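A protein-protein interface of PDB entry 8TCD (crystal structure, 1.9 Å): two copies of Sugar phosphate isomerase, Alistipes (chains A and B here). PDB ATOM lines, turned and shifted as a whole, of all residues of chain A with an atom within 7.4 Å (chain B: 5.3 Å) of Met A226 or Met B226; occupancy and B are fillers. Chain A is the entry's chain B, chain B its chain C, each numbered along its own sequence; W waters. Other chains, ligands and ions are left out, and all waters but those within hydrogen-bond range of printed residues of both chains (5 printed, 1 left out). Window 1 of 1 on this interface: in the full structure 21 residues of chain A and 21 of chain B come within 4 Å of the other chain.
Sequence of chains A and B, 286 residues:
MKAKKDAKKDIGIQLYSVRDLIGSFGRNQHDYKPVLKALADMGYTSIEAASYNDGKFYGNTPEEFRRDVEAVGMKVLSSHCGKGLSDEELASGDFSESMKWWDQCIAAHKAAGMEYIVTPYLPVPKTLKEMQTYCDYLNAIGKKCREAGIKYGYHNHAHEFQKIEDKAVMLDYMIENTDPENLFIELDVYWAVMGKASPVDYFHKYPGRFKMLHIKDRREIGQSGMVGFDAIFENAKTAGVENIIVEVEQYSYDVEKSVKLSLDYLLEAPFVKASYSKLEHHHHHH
Water W1 lies within hydrogen-bond range of the backbone carbonyl oxygen (O) of Val B227 (2.8 Å) and the side-chain carboxylate (OD1) of Asp A230 (2.8 Å).
Water W2 lies within hydrogen-bond range of NZ of Lys A196 (2.8 Å), O of Met A194 (2.9 Å), NZ of Lys B196 (3.0 Å) and O of Met B194 (3.1 Å).
Water W3 bridges the backbone NH of Ser B198 (3.0 Å) and the guanidinium group of Arg A218 (3.4 Å).
OG of Ser A224 is in hydrogen-bond range of N of Met A226, 2.8 Å away.
The side-chain hydroxyl of Ser A198 lies close to the backbone NH of Val A200 (3.3 Å).
The guanidinium group of Arg A218 lies close to the side-chain sulfur of Met A226, at 3.5 Å.
NH2 of Arg A218 is in hydrogen-bond range of SD of Met A194 (3.6 Å).
O of Ala A192 is in hydrogen-bond range of N of Ala A197 (2.9 Å).
O of Met B226 lies close to O of Met A226, 3.2 Å away.
The backbone NH of Val A200 sits at hydrogen-bond distance from the backbone carbonyl oxygen of Ser B224, 3.1 Å away.
The backbone carbonyl oxygen (O) of Ala B197 sits close to the side-chain sulfur (SD) of Met A226 (3.7 Å).
The backbone carbonyl oxygen (O) of Ser A224 is in hydrogen-bond range of the side-chain hydroxyl (OG) of Ser B198 (2.8 Å).
The backbone NH of Gly B228 lies within hydrogen-bond range of the backbone carbonyl oxygen of Gly A225, at 2.9 Å.
The side-chain hydroxyl (OG) of Ser A198 lies within hydrogen-bond range of the backbone carbonyl oxygen (O) of Ser B224 (2.7 Å).
The backbone carbonyl oxygen of Ser A224 lies close to the backbone nitrogen of Pro B199 (3.5 Å).
O of Ala A197 lies close to SD of Met B226 (3.7 Å).
NH2 of Arg A218 sits at hydrogen-bond distance from O of Lys B196 (2.8 Å).
The backbone carbonyl oxygen (O) of Lys A196 lies within hydrogen-bond range of the guanidinium group (NH2) of Arg B218 (2.9 Å).
N of Gly A228 is in hydrogen-bond range of O of Gly B225, 2.8 Å away.
CG1 of Val A193 touches CG1 of Val B193, 3.2 Å away.
Met A194 touches Lys B196.
Pro A199 touches Ser B224.
Met B226 touches Pro A199 (CG to CD, 3.997 Å).
Gly A225 touches Val B227 (O to C, 3.9 Å).
Lys B196 touches Met A226.
CA of Ser B198 touches CG of Met A226, 3.7 Å away.
Met A226 touches Pro B199 (CG to CD, 3.97 Å).
CA of Gly A228 touches O of Val B227, 3.1 Å away.
CB of Ala A231 touches N of Gly B225, at 3.6 Å.
Val B193 touches its own counterpart, Val A193.
Ser A198 touches Met B226, and with the chains exchanged Met A226 touches Ser B198.
Pro A199 touches Ser B224, and with the chains exchanged Ser A224 touches Pro B199.
Gly A225 touches Gly B228, and with the chains exchanged Gly A228 touches Gly B225.
Of the 36 pairs that touch across the chains among the printed residues, 33 have their exchanged pair printed and touching as well.
Hydrophobic or aromatic side chains of chain B within 4 Å of the printed part of chain A: Val B193, Met B194, Pro B199 and Met B226.
Of the 26 printed residues of chain A, 15 touch a printed residue of chain B.
Hydrophobic or aromatic side chains of chain A within 4 Å of the printed part of chain B: Val A193, Met A194, Pro A199, Val A200, Met A226, Ala A231 and Ile A232.
Among the printed residues, 36 pairs touch across the chains.
Met A226 touches six residues of chain B.
Of the printed residues of chain A, Val B193 touches Val A193, Gly A225 and Met A226.
Of the printed residues of chain A, Val B227 touches Gly A225, Val A227 and Gly A228.
Of the printed residues of chain A, Met B194 touches Lys A196 (3.9 Å).
Lys A216 touches none of the printed residues of chain B.
The nearest printed residue of chain A that does not touch Met B226 is Gly A228 (4.03 Å).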
ATOM      1  N   VAL A 189      11.004 -19.998  -4.660  1.00  0.00           N
ATOM      2  CA  VAL A 189       9.783 -20.648  -5.088  1.00  0.00           C
ATOM      3  C   VAL A 189       8.593 -19.700  -4.944  1.00  0.00           C
ATOM      4  O   VAL A 189       7.640 -19.804  -5.700  1.00  0.00           O
ATOM      5  CB  VAL A 189       9.554 -21.967  -4.330  1.00  0.00           C
ATOM      6  CG1 VAL A 189      10.617 -22.998  -4.718  1.00  0.00           C
ATOM      7  CG2 VAL A 189       9.508 -21.777  -2.820  1.00  0.00           C
ATOM      8  N   TYR A 190       8.662 -18.788  -3.972  1.00  0.00           N
ATOM      9  CA  TYR A 190       7.621 -17.793  -3.793  1.00  0.00           C
ATOM     10  C   TYR A 190       7.631 -16.808  -4.954  1.00  0.00           C
ATOM     11  O   TYR A 190       6.570 -16.554  -5.514  1.00  0.00           O
ATOM     12  CB  TYR A 190       7.781 -17.006  -2.496  1.00  0.00           C
ATOM     13  CG  TYR A 190       6.784 -15.866  -2.343  1.00  0.00           C
ATOM     14  CD1 TYR A 190       5.455 -16.099  -1.975  1.00  0.00           C
ATOM     15  CD2 TYR A 190       7.177 -14.551  -2.547  1.00  0.00           C
ATOM     16  CE1 TYR A 190       4.562 -15.056  -1.817  1.00  0.00           C
ATOM     17  CE2 TYR A 190       6.297 -13.496  -2.374  1.00  0.00           C
ATOM     18  CZ  TYR A 190       4.995 -13.750  -1.999  1.00  0.00           C
ATOM     19  OH  TYR A 190       4.176 -12.685  -1.872  1.00  0.00           O
ATOM     20  N   ALA A 192       8.905 -17.254  -7.848  1.00  0.00           N
ATOM     21  CA  ALA A 192       8.533 -18.003  -9.045  1.00  0.00           C
ATOM     22  C   ALA A 192       7.019 -18.000  -9.180  1.00  0.00           C
ATOM     23  O   ALA A 192       6.500 -17.647 -10.235  1.00  0.00           O
ATOM     24  CB  ALA A 192       9.048 -19.423  -9.042  1.00  0.00           C
ATOM     25  N   VAL A 193       6.323 -18.384  -8.101  1.00  0.00           N
ATOM     26  CA  VAL A 193       4.864 -18.397  -8.104  1.00  0.00           C
ATOM     27  C   VAL A 193       4.334 -16.997  -8.406  1.00  0.00           C
ATOM     28  O   VAL A 193       3.394 -16.833  -9.178  1.00  0.00           O
ATOM     29  CB  VAL A 193       4.329 -18.954  -6.766  1.00  0.00           C
ATOM     30  CG1 VAL A 193       2.838 -18.743  -6.573  1.00  0.00           C
ATOM     31  CG2 VAL A 193       4.651 -20.433  -6.629  1.00  0.00           C
ATOM     32  N   MET A 194       4.948 -15.985  -7.799  1.00  0.00           N
ATOM     33  CA  MET A 194       4.563 -14.610  -8.041  1.00  0.00           C
ATOM     34  C   MET A 194       4.753 -14.241  -9.518  1.00  0.00           C
ATOM     35  O   MET A 194       4.043 -13.389 -10.035  1.00  0.00           O
ATOM     36  CB  MET A 194       5.334 -13.694  -7.089  1.00  0.00           C
ATOM     37  CG  MET A 194       4.828 -13.765  -5.659  1.00  0.00           C
ATOM     38  SD  MET A 194       3.204 -13.011  -5.418  1.00  0.00           S
ATOM     39  CE  MET A 194       3.862 -11.340  -5.291  1.00  0.00           C
ATOM     40  N   GLY A 195       5.691 -14.902 -10.202  1.00  0.00           N
ATOM     41  CA  GLY A 195       5.890 -14.756 -11.635  1.00  0.00           C
ATOM     42  C   GLY A 195       5.072 -15.727 -12.502  1.00  0.00           C
ATOM     43  O   GLY A 195       5.369 -15.851 -13.690  1.00  0.00           O
ATOM     44  N   LYS A 196       4.068 -16.389 -11.908  1.00  0.00           N
ATOM     45  CA  LYS A 196       3.161 -17.330 -12.552  1.00  0.00           C
ATOM     46  C   LYS A 196       3.896 -18.575 -13.038  1.00  0.00           C
ATOM     47  O   LYS A 196       3.420 -19.256 -13.936  1.00  0.00           O
ATOM     48  CB  LYS A 196       2.365 -16.699 -13.700  1.00  0.00           C
ATOM     49  CG  LYS A 196       1.542 -15.460 -13.294  1.00  0.00           C
ATOM     50  CD  LYS A 196       0.932 -14.726 -14.497  1.00  0.00           C
ATOM     51  CE  LYS A 196      -0.077 -13.664 -14.122  1.00  0.00           C
ATOM     52  NZ  LYS A 196       0.548 -12.560 -13.399  1.00  0.00           N
ATOM     53  N   ALA A 197       5.049 -18.881 -12.435  1.00  0.00           N
ATOM     54  CA  ALA A 197       5.832 -20.026 -12.851  1.00  0.00           C
ATOM     55  C   ALA A 197       5.548 -21.182 -11.902  1.00  0.00           C
ATOM     56  O   ALA A 197       5.355 -20.960 -10.700  1.00  0.00           O
ATOM     57  CB  ALA A 197       7.309 -19.703 -12.873  1.00  0.00           C
ATOM     58  N   SER A 198       5.509 -22.394 -12.476  1.00  0.00           N
ATOM     59  CA  SER A 198       5.443 -23.607 -11.697  1.00  0.00           C
ATOM     60  C   SER A 198       6.856 -24.023 -11.299  1.00  0.00           C
ATOM     61  O   SER A 198       7.638 -24.456 -12.147  1.00  0.00           O
ATOM     62  CB  SER A 198       4.750 -24.755 -12.436  1.00  0.00           C
ATOM     63  OG  SER A 198       5.001 -25.981 -11.764  1.00  0.00           O
ATOM     64  N   PRO A 199       7.194 -24.012  -9.989  1.00  0.00           N
ATOM     65  CA  PRO A 199       8.467 -24.575  -9.536  1.00  0.00           C
ATOM     66  C   PRO A 199       8.702 -25.992 -10.041  1.00  0.00           C
ATOM     67  O   PRO A 199       9.771 -26.299 -10.548  1.00  0.00           O
ATOM     68  CB  PRO A 199       8.405 -24.495  -7.995  1.00  0.00           C
ATOM     69  CG  PRO A 199       7.422 -23.383  -7.734  1.00  0.00           C
ATOM     70  CD  PRO A 199       6.391 -23.471  -8.876  1.00  0.00           C
ATOM     71  N   VAL A 200       7.678 -26.838  -9.974  1.00  0.00           N
ATOM     72  CA  VAL A 200       7.874 -28.227 -10.352  1.00  0.00           C
ATOM     73  C   VAL A 200       8.081 -28.351 -11.859  1.00  0.00           C
ATOM     74  O   VAL A 200       8.891 -29.166 -12.290  1.00  0.00           O
ATOM     75  CB  VAL A 200       6.719 -29.124  -9.886  1.00  0.00           C
ATOM     76  CG1 VAL A 200       6.797 -30.515 -10.522  1.00  0.00           C
ATOM     77  CG2 VAL A 200       6.664 -29.193  -8.366  1.00  0.00           C
ATOM     78  N   ASP A 201       7.355 -27.568 -12.672  1.00  0.00           N
ATOM     79  CA  ASP A 201       7.576 -27.639 -14.105  1.00  0.00           C
ATOM     80  C   ASP A 201       8.975 -27.159 -14.481  1.00  0.00           C
ATOM     81  O   ASP A 201       9.583 -27.721 -15.405  1.00  0.00           O
ATOM     82  CB  ASP A 201       6.537 -26.882 -14.904  1.00  0.00           C
ATOM     83  CG  ASP A 201       5.138 -27.453 -14.814  1.00  0.00           C
ATOM     84  OD1 ASP A 201       5.009 -28.624 -14.386  1.00  0.00           O
ATOM     85  OD2 ASP A 201       4.188 -26.689 -15.122  1.00  0.00           O
ATOM     86  N   LYS A 216      10.658 -19.616   0.583  1.00  0.00           N
ATOM     87  CA  LYS A 216      10.070 -18.350   0.931  1.00  0.00           C
ATOM     88  C   LYS A 216       8.571 -18.480   0.730  1.00  0.00           C
ATOM     89  O   LYS A 216       8.115 -19.319  -0.044  1.00  0.00           O
ATOM     90  CB  LYS A 216      10.646 -17.231   0.063  1.00  0.00           C
ATOM     91  CG  LYS A 216      10.167 -15.828   0.431  1.00  0.00           C
ATOM     92  CD  LYS A 216      10.611 -14.714  -0.507  1.00  0.00           C
ATOM     93  CE  LYS A 216      10.163 -13.364   0.000  1.00  0.00           C
ATOM     94  NZ  LYS A 216       8.713 -13.250   0.242  1.00  0.00           N
ATOM     95  N   ASP A 217       7.831 -17.644   1.456  1.00  0.00           N
ATOM     96  CA  ASP A 217       6.389 -17.535   1.346  1.00  0.00           C
ATOM     97  C   ASP A 217       6.088 -16.047   1.530  1.00  0.00           C
ATOM     98  O   ASP A 217       7.007 -15.243   1.591  1.00  0.00           O
ATOM     99  CB  ASP A 217       5.731 -18.559   2.264  1.00  0.00           C
ATOM    100  CG  ASP A 217       4.287 -18.921   1.953  1.00  0.00           C
ATOM    101  OD1 ASP A 217       3.623 -18.159   1.227  1.00  0.00           O
ATOM    102  OD2 ASP A 217       3.809 -19.929   2.488  1.00  0.00           O
ATOM    103  N   ARG A 218       4.809 -15.662   1.566  1.00  0.00           N
ATOM    104  CA  ARG A 218       4.477 -14.257   1.738  1.00  0.00           C
ATOM    105  C   ARG A 218       5.051 -13.747   3.062  1.00  0.00           C
ATOM    106  O   ARG A 218       5.735 -12.725   3.095  1.00  0.00           O
ATOM    107  CB  ARG A 218       2.970 -14.004   1.693  1.00  0.00           C
ATOM    108  CG  ARG A 218       2.685 -12.515   1.822  1.00  0.00           C
ATOM    109  CD  ARG A 218       1.481 -12.053   1.047  1.00  0.00           C
ATOM    110  NE  ARG A 218       1.743 -12.039  -0.398  1.00  0.00           N
ATOM    111  CZ  ARG A 218       0.826 -11.885  -1.354  1.00  0.00           C
ATOM    112  NH1 ARG A 218      -0.441 -11.677  -1.047  1.00  0.00           N
ATOM    113  NH2 ARG A 218       1.184 -11.937  -2.625  1.00  0.00           N
ATOM    114  N   GLY A 222       4.705 -21.689   4.751  1.00  0.00           N
ATOM    115  CA  GLY A 222       3.555 -22.567   4.816  1.00  0.00           C
ATOM    116  C   GLY A 222       2.277 -21.900   5.322  1.00  0.00           C
ATOM    117  O   GLY A 222       1.308 -22.620   5.522  1.00  0.00           O
ATOM    118  N   GLN A 223       2.266 -20.577   5.530  1.00  0.00           N
ATOM    119  CA  GLN A 223       1.128 -19.863   6.113  1.00  0.00           C
ATOM    120  C   GLN A 223       0.111 -19.413   5.058  1.00  0.00           C
ATOM    121  O   GLN A 223      -1.059 -19.316   5.376  1.00  0.00           O
ATOM    122  CB  GLN A 223       1.611 -18.628   6.888  1.00  0.00           C
ATOM    123  CG  GLN A 223       0.551 -17.625   7.363  1.00  0.00           C
ATOM    124  CD  GLN A 223       0.210 -16.539   6.357  1.00  0.00           C
ATOM    125  OE1 GLN A 223       1.088 -15.982   5.683  1.00  0.00           O
ATOM    126  NE2 GLN A 223      -1.071 -16.194   6.263  1.00  0.00           N
ATOM    127  N   SER A 224       0.546 -19.075   3.835  1.00  0.00           N
ATOM    128  CA  SER A 224      -0.222 -18.179   2.963  1.00  0.00           C
ATOM    129  C   SER A 224      -1.260 -18.920   2.120  1.00  0.00           C
ATOM    130  O   SER A 224      -2.279 -18.342   1.718  1.00  0.00           O
ATOM    131  CB  SER A 224       0.690 -17.412   2.059  1.00  0.00           C
ATOM    132  OG  SER A 224       1.255 -18.229   1.049  1.00  0.00           O
ATOM    133  N   GLY A 225      -0.920 -20.165   1.759  1.00  0.00           N
ATOM    134  CA  GLY A 225      -1.652 -20.914   0.755  1.00  0.00           C
ATOM    135  C   GLY A 225      -1.124 -20.690  -0.659  1.00  0.00           C
ATOM    136  O   GLY A 225      -1.707 -21.209  -1.616  1.00  0.00           O
ATOM    137  N   MET A 226      -0.040 -19.911  -0.799  1.00  0.00           N
ATOM    138  CA  MET A 226       0.414 -19.485  -2.115  1.00  0.00           C
ATOM    139  C   MET A 226       1.548 -20.378  -2.618  1.00  0.00           C
ATOM    140  O   MET A 226       2.043 -20.165  -3.728  1.00  0.00           O
ATOM    141  CB  MET A 226       0.904 -18.029  -2.108  1.00  0.00           C
ATOM    142  CG  MET A 226      -0.156 -17.003  -1.737  1.00  0.00           C
ATOM    143  SD  MET A 226       0.482 -15.333  -1.945  1.00  0.00           S
ATOM    144  CE  MET A 226       0.379 -15.072  -3.716  1.00  0.00           C
ATOM    145  N   VAL A 227       1.999 -21.345  -1.799  1.00  0.00           N
ATOM    146  CA  VAL A 227       3.180 -22.100  -2.172  1.00  0.00           C
ATOM    147  C   VAL A 227       2.957 -23.566  -1.839  1.00  0.00           C
ATOM    148  O   VAL A 227       2.729 -23.924  -0.686  1.00  0.00           O
ATOM    149  CB  VAL A 227       4.512 -21.611  -1.575  1.00  0.00           C
ATOM    150  CG1 VAL A 227       5.658 -22.478  -2.075  1.00  0.00           C
ATOM    151  CG2 VAL A 227       4.824 -20.153  -1.918  1.00  0.00           C
ATOM    152  N   GLY A 228       3.092 -24.413  -2.865  1.00  0.00           N
ATOM    153  CA  GLY A 228       2.962 -25.850  -2.673  1.00  0.00           C
ATOM    154  C   GLY A 228       4.275 -26.533  -2.288  1.00  0.00           C
ATOM    155  O   GLY A 228       4.875 -27.230  -3.113  1.00  0.00           O
ATOM    156  N   PHE A 229       4.659 -26.428  -1.004  1.00  0.00           N
ATOM    157  CA  PHE A 229       5.928 -26.975  -0.524  1.00  0.00           C
ATOM    158  C   PHE A 229       5.956 -28.495  -0.715  1.00  0.00           C
ATOM    159  O   PHE A 229       6.986 -29.043  -1.132  1.00  0.00           O
ATOM    160  CB  PHE A 229       6.225 -26.523   0.922  1.00  0.00           C
ATOM    161  CG  PHE A 229       6.458 -25.024   0.998  1.00  0.00           C
ATOM    162  CD1 PHE A 229       7.612 -24.483   0.457  1.00  0.00           C
ATOM    163  CD2 PHE A 229       5.527 -24.168   1.556  1.00  0.00           C
ATOM    164  CE1 PHE A 229       7.834 -23.121   0.476  1.00  0.00           C
ATOM    165  CE2 PHE A 229       5.768 -22.809   1.600  1.00  0.00           C
ATOM    166  CZ  PHE A 229       6.918 -22.289   1.063  1.00  0.00           C
ATOM    167  N   ASP A 230       4.813 -29.163  -0.478  1.00  0.00           N
ATOM    168  CA  ASP A 230       4.702 -30.606  -0.665  1.00  0.00           C
ATOM    169  C   ASP A 230       5.213 -30.999  -2.051  1.00  0.00           C
ATOM    170  O   ASP A 230       6.157 -31.777  -2.176  1.00  0.00           O
ATOM    171  CB  ASP A 230       3.306 -31.137  -0.334  1.00  0.00           C
ATOM    172  CG  ASP A 230       2.101 -30.585  -1.090  1.00  0.00           C
ATOM    173  OD1 ASP A 230       2.203 -29.540  -1.786  1.00  0.00           O
ATOM    174  OD2 ASP A 230       1.040 -31.199  -0.964  1.00  0.00           O
ATOM    175  N   ALA A 231       4.625 -30.410  -3.093  1.00  0.00           N
ATOM    176  CA  ALA A 231       4.971 -30.723  -4.466  1.00  0.00           C
ATOM    177  C   ALA A 231       6.435 -30.408  -4.747  1.00  0.00           C
ATOM    178  O   ALA A 231       7.125 -31.176  -5.415  1.00  0.00           O
ATOM    179  CB  ALA A 231       4.068 -29.958  -5.393  1.00  0.00           C
ATOM    180  N   ILE A 232       6.884 -29.252  -4.260  1.00  0.00           N
ATOM    181  CA  ILE A 232       8.238 -28.793  -4.501  1.00  0.00           C
ATOM    182  C   ILE A 232       9.234 -29.822  -3.964  1.00  0.00           C
ATOM    183  O   ILE A 232      10.147 -30.269  -4.659  1.00  0.00           O
ATOM    184  CB  ILE A 232       8.427 -27.393  -3.878  1.00  0.00           C
ATOM    185  CG1 ILE A 232       7.609 -26.346  -4.664  1.00  0.00           C
ATOM    186  CG2 ILE A 232       9.909 -27.022  -3.777  1.00  0.00           C
ATOM    187  CD1 ILE A 232       7.537 -24.966  -4.051  1.00  0.00           C
ATOM    188  N   TYR B 190      -6.266 -21.516  -6.983  1.00  0.00           N
ATOM    189  CA  TYR B 190      -5.237 -21.362  -7.996  1.00  0.00           C
ATOM    190  C   TYR B 190      -5.260 -19.939  -8.557  1.00  0.00           C
ATOM    191  O   TYR B 190      -4.231 -19.291  -8.635  1.00  0.00           O
ATOM    192  CB  TYR B 190      -5.411 -22.356  -9.147  1.00  0.00           C
ATOM    193  CG  TYR B 190      -4.455 -22.150 -10.313  1.00  0.00           C
ATOM    194  CD1 TYR B 190      -3.103 -22.471 -10.208  1.00  0.00           C
ATOM    195  CD2 TYR B 190      -4.909 -21.625 -11.516  1.00  0.00           C
ATOM    196  CE1 TYR B 190      -2.242 -22.293 -11.275  1.00  0.00           C
ATOM    197  CE2 TYR B 190      -4.050 -21.416 -12.584  1.00  0.00           C
ATOM    198  CZ  TYR B 190      -2.725 -21.783 -12.473  1.00  0.00           C
ATOM    199  OH  TYR B 190      -1.896 -21.629 -13.542  1.00  0.00           O
ATOM    200  N   VAL B 193      -4.006 -17.315  -6.312  1.00  0.00           N
ATOM    201  CA  VAL B 193      -2.549 -17.282  -6.295  1.00  0.00           C
ATOM    202  C   VAL B 193      -2.047 -16.588  -7.551  1.00  0.00           C
ATOM    203  O   VAL B 193      -1.137 -15.769  -7.475  1.00  0.00           O
ATOM    204  CB  VAL B 193      -1.900 -18.671  -6.154  1.00  0.00           C
ATOM    205  CG1 VAL B 193      -0.395 -18.603  -6.377  1.00  0.00           C
ATOM    206  CG2 VAL B 193      -2.217 -19.284  -4.796  1.00  0.00           C
ATOM    207  N   MET B 194      -2.644 -16.920  -8.698  1.00  0.00           N
ATOM    208  CA  MET B 194      -2.217 -16.336  -9.952  1.00  0.00           C
ATOM    209  C   MET B 194      -2.428 -14.837  -9.930  1.00  0.00           C
ATOM    210  O   MET B 194      -1.759 -14.146 -10.683  1.00  0.00           O
ATOM    211  CB  MET B 194      -2.977 -16.918 -11.155  1.00  0.00           C
ATOM    212  CG  MET B 194      -2.513 -18.338 -11.530  1.00  0.00           C
ATOM    213  SD  MET B 194      -0.872 -18.321 -12.300  1.00  0.00           S
ATOM    214  CE  MET B 194      -1.327 -17.962 -14.004  1.00  0.00           C
ATOM    215  N   LYS B 196      -1.866 -13.076  -7.340  1.00  0.00           N
ATOM    216  CA  LYS B 196      -0.941 -12.667  -6.289  1.00  0.00           C
ATOM    217  C   LYS B 196      -1.648 -12.534  -4.942  1.00  0.00           C
ATOM    218  O   LYS B 196      -1.169 -11.808  -4.076  1.00  0.00           O
ATOM    219  CB  LYS B 196      -0.223 -11.358  -6.654  1.00  0.00           C
ATOM    220  CG  LYS B 196       0.619 -11.399  -7.907  1.00  0.00           C
ATOM    221  CD  LYS B 196       1.368 -10.086  -8.116  1.00  0.00           C
ATOM    222  CE  LYS B 196       2.418 -10.122  -9.167  1.00  0.00           C
ATOM    223  NZ  LYS B 196       1.818 -10.259 -10.491  1.00  0.00           N
ATOM    224  N   ALA B 197      -2.793 -13.204  -4.771  1.00  0.00           N
ATOM    225  CA  ALA B 197      -3.558 -13.106  -3.537  1.00  0.00           C
ATOM    226  C   ALA B 197      -3.216 -14.310  -2.658  1.00  0.00           C
ATOM    227  O   ALA B 197      -3.011 -15.419  -3.173  1.00  0.00           O
ATOM    228  CB  ALA B 197      -5.049 -13.038  -3.833  1.00  0.00           C
ATOM    229  N   SER B 198      -3.077 -14.067  -1.350  1.00  0.00           N
ATOM    230  CA  SER B 198      -3.003 -15.141  -0.367  1.00  0.00           C
ATOM    231  C   SER B 198      -4.401 -15.662  -0.076  1.00  0.00           C
ATOM    232  O   SER B 198      -5.220 -14.911   0.450  1.00  0.00           O
ATOM    233  CB  SER B 198      -2.350 -14.654   0.928  1.00  0.00           C
ATOM    234  OG  SER B 198      -2.518 -15.604   1.978  1.00  0.00           O
ATOM    235  N   PRO B 199      -4.738 -16.943  -0.342  1.00  0.00           N
ATOM    236  CA  PRO B 199      -6.052 -17.442   0.045  1.00  0.00           C
ATOM    237  C   PRO B 199      -6.314 -17.286   1.535  1.00  0.00           C
ATOM    238  O   PRO B 199      -7.414 -16.924   1.934  1.00  0.00           O
ATOM    239  CB  PRO B 199      -6.068 -18.900  -0.415  1.00  0.00           C
ATOM    240  CG  PRO B 199      -5.072 -18.926  -1.570  1.00  0.00           C
ATOM    241  CD  PRO B 199      -3.974 -17.919  -1.148  1.00  0.00           C
ATOM    242  N   ASP B 217      -5.424 -26.343  -9.520  1.00  0.00           N
ATOM    243  CA  ASP B 217      -3.987 -26.175  -9.643  1.00  0.00           C
ATOM    244  C   ASP B 217      -3.736 -25.867 -11.116  1.00  0.00           C
ATOM    245  O   ASP B 217      -4.682 -25.598 -11.848  1.00  0.00           O
ATOM    246  CB  ASP B 217      -3.271 -27.377  -9.046  1.00  0.00           C
ATOM    247  CG  ASP B 217      -1.843 -27.156  -8.566  1.00  0.00           C
ATOM    248  OD1 ASP B 217      -1.210 -26.184  -9.055  1.00  0.00           O
ATOM    249  OD2 ASP B 217      -1.382 -27.934  -7.693  1.00  0.00           O
ATOM    250  N   ARG B 218      -2.483 -25.865 -11.568  1.00  0.00           N
ATOM    251  CA  ARG B 218      -2.222 -25.613 -12.978  1.00  0.00           C
ATOM    252  C   ARG B 218      -2.755 -26.804 -13.797  1.00  0.00           C
ATOM    253  O   ARG B 218      -3.495 -26.655 -14.776  1.00  0.00           O
ATOM    254  CB  ARG B 218      -0.734 -25.294 -13.152  1.00  0.00           C
ATOM    255  CG  ARG B 218      -0.376 -25.034 -14.604  1.00  0.00           C
ATOM    256  CD  ARG B 218       0.934 -24.274 -14.806  1.00  0.00           C
ATOM    257  NE  ARG B 218       0.660 -22.935 -14.281  1.00  0.00           N
ATOM    258  CZ  ARG B 218       1.418 -21.874 -14.404  1.00  0.00           C
ATOM    259  NH1 ARG B 218       2.661 -22.011 -14.819  1.00  0.00           N
ATOM    260  NH2 ARG B 218       0.930 -20.693 -14.053  1.00  0.00           N
ATOM    261  N   SER B 224       1.991 -28.826  -9.000  1.00  0.00           N
ATOM    262  CA  SER B 224       2.707 -27.721  -9.619  1.00  0.00           C
ATOM    263  C   SER B 224       3.725 -27.082  -8.693  1.00  0.00           C
ATOM    264  O   SER B 224       4.678 -26.456  -9.172  1.00  0.00           O
ATOM    265  CB  SER B 224       1.764 -26.658 -10.065  1.00  0.00           C
ATOM    266  OG  SER B 224       1.260 -25.891  -8.978  1.00  0.00           O
ATOM    267  N   GLY B 225       3.403 -27.085  -7.400  1.00  0.00           N
ATOM    268  CA  GLY B 225       4.138 -26.331  -6.404  1.00  0.00           C
ATOM    269  C   GLY B 225       3.619 -24.900  -6.231  1.00  0.00           C
ATOM    270  O   GLY B 225       4.206 -24.157  -5.454  1.00  0.00           O
ATOM    271  N   MET B 226       2.538 -24.542  -6.930  1.00  0.00           N
ATOM    272  CA  MET B 226       2.015 -23.187  -6.932  1.00  0.00           C
ATOM    273  C   MET B 226       0.882 -22.988  -5.925  1.00  0.00           C
ATOM    274  O   MET B 226       0.371 -21.869  -5.813  1.00  0.00           O
ATOM    275  CB  MET B 226       1.455 -22.787  -8.305  1.00  0.00           C
ATOM    276  CG  MET B 226       2.480 -22.863  -9.431  1.00  0.00           C
ATOM    277  SD  MET B 226       1.842 -22.199 -10.981  1.00  0.00           S
ATOM    278  CE  MET B 226       1.832 -20.429 -10.644  1.00  0.00           C
ATOM    279  N   VAL B 227       0.418 -24.053  -5.263  1.00  0.00           N
ATOM    280  CA  VAL B 227      -0.745 -23.912  -4.396  1.00  0.00           C
ATOM    281  C   VAL B 227      -0.478 -24.609  -3.070  1.00  0.00           C
ATOM    282  O   VAL B 227      -0.160 -25.806  -3.020  1.00  0.00           O
ATOM    283  CB  VAL B 227      -2.047 -24.420  -5.037  1.00  0.00           C
ATOM    284  CG1 VAL B 227      -3.219 -24.186  -4.098  1.00  0.00           C
ATOM    285  CG2 VAL B 227      -2.314 -23.743  -6.380  1.00  0.00           C
ATOM    286  N   GLY B 228      -0.604 -23.817  -1.996  1.00  0.00           N
ATOM    287  CA  GLY B 228      -0.406 -24.310  -0.647  1.00  0.00           C
ATOM    288  C   GLY B 228      -1.701 -24.859  -0.049  1.00  0.00           C
ATOM    289  O   GLY B 228      -2.282 -24.241   0.839  1.00  0.00           O
HETATM  290  O   HOH W   1       0.546 -28.390  -3.734  1.00  0.00           O
HETATM  291  O   HOH W   2       1.186 -13.225 -10.749  1.00  0.00           O
HETATM  292  O   HOH W   3      -3.812 -11.317  -0.419  1.00  0.00           O
HETATM  293  O   HOH W   4      -0.045 -14.565   3.478  1.00  0.00           O
HETATM  294  O   HOH W   5       4.093 -24.179 -16.022  1.00  0.00           O
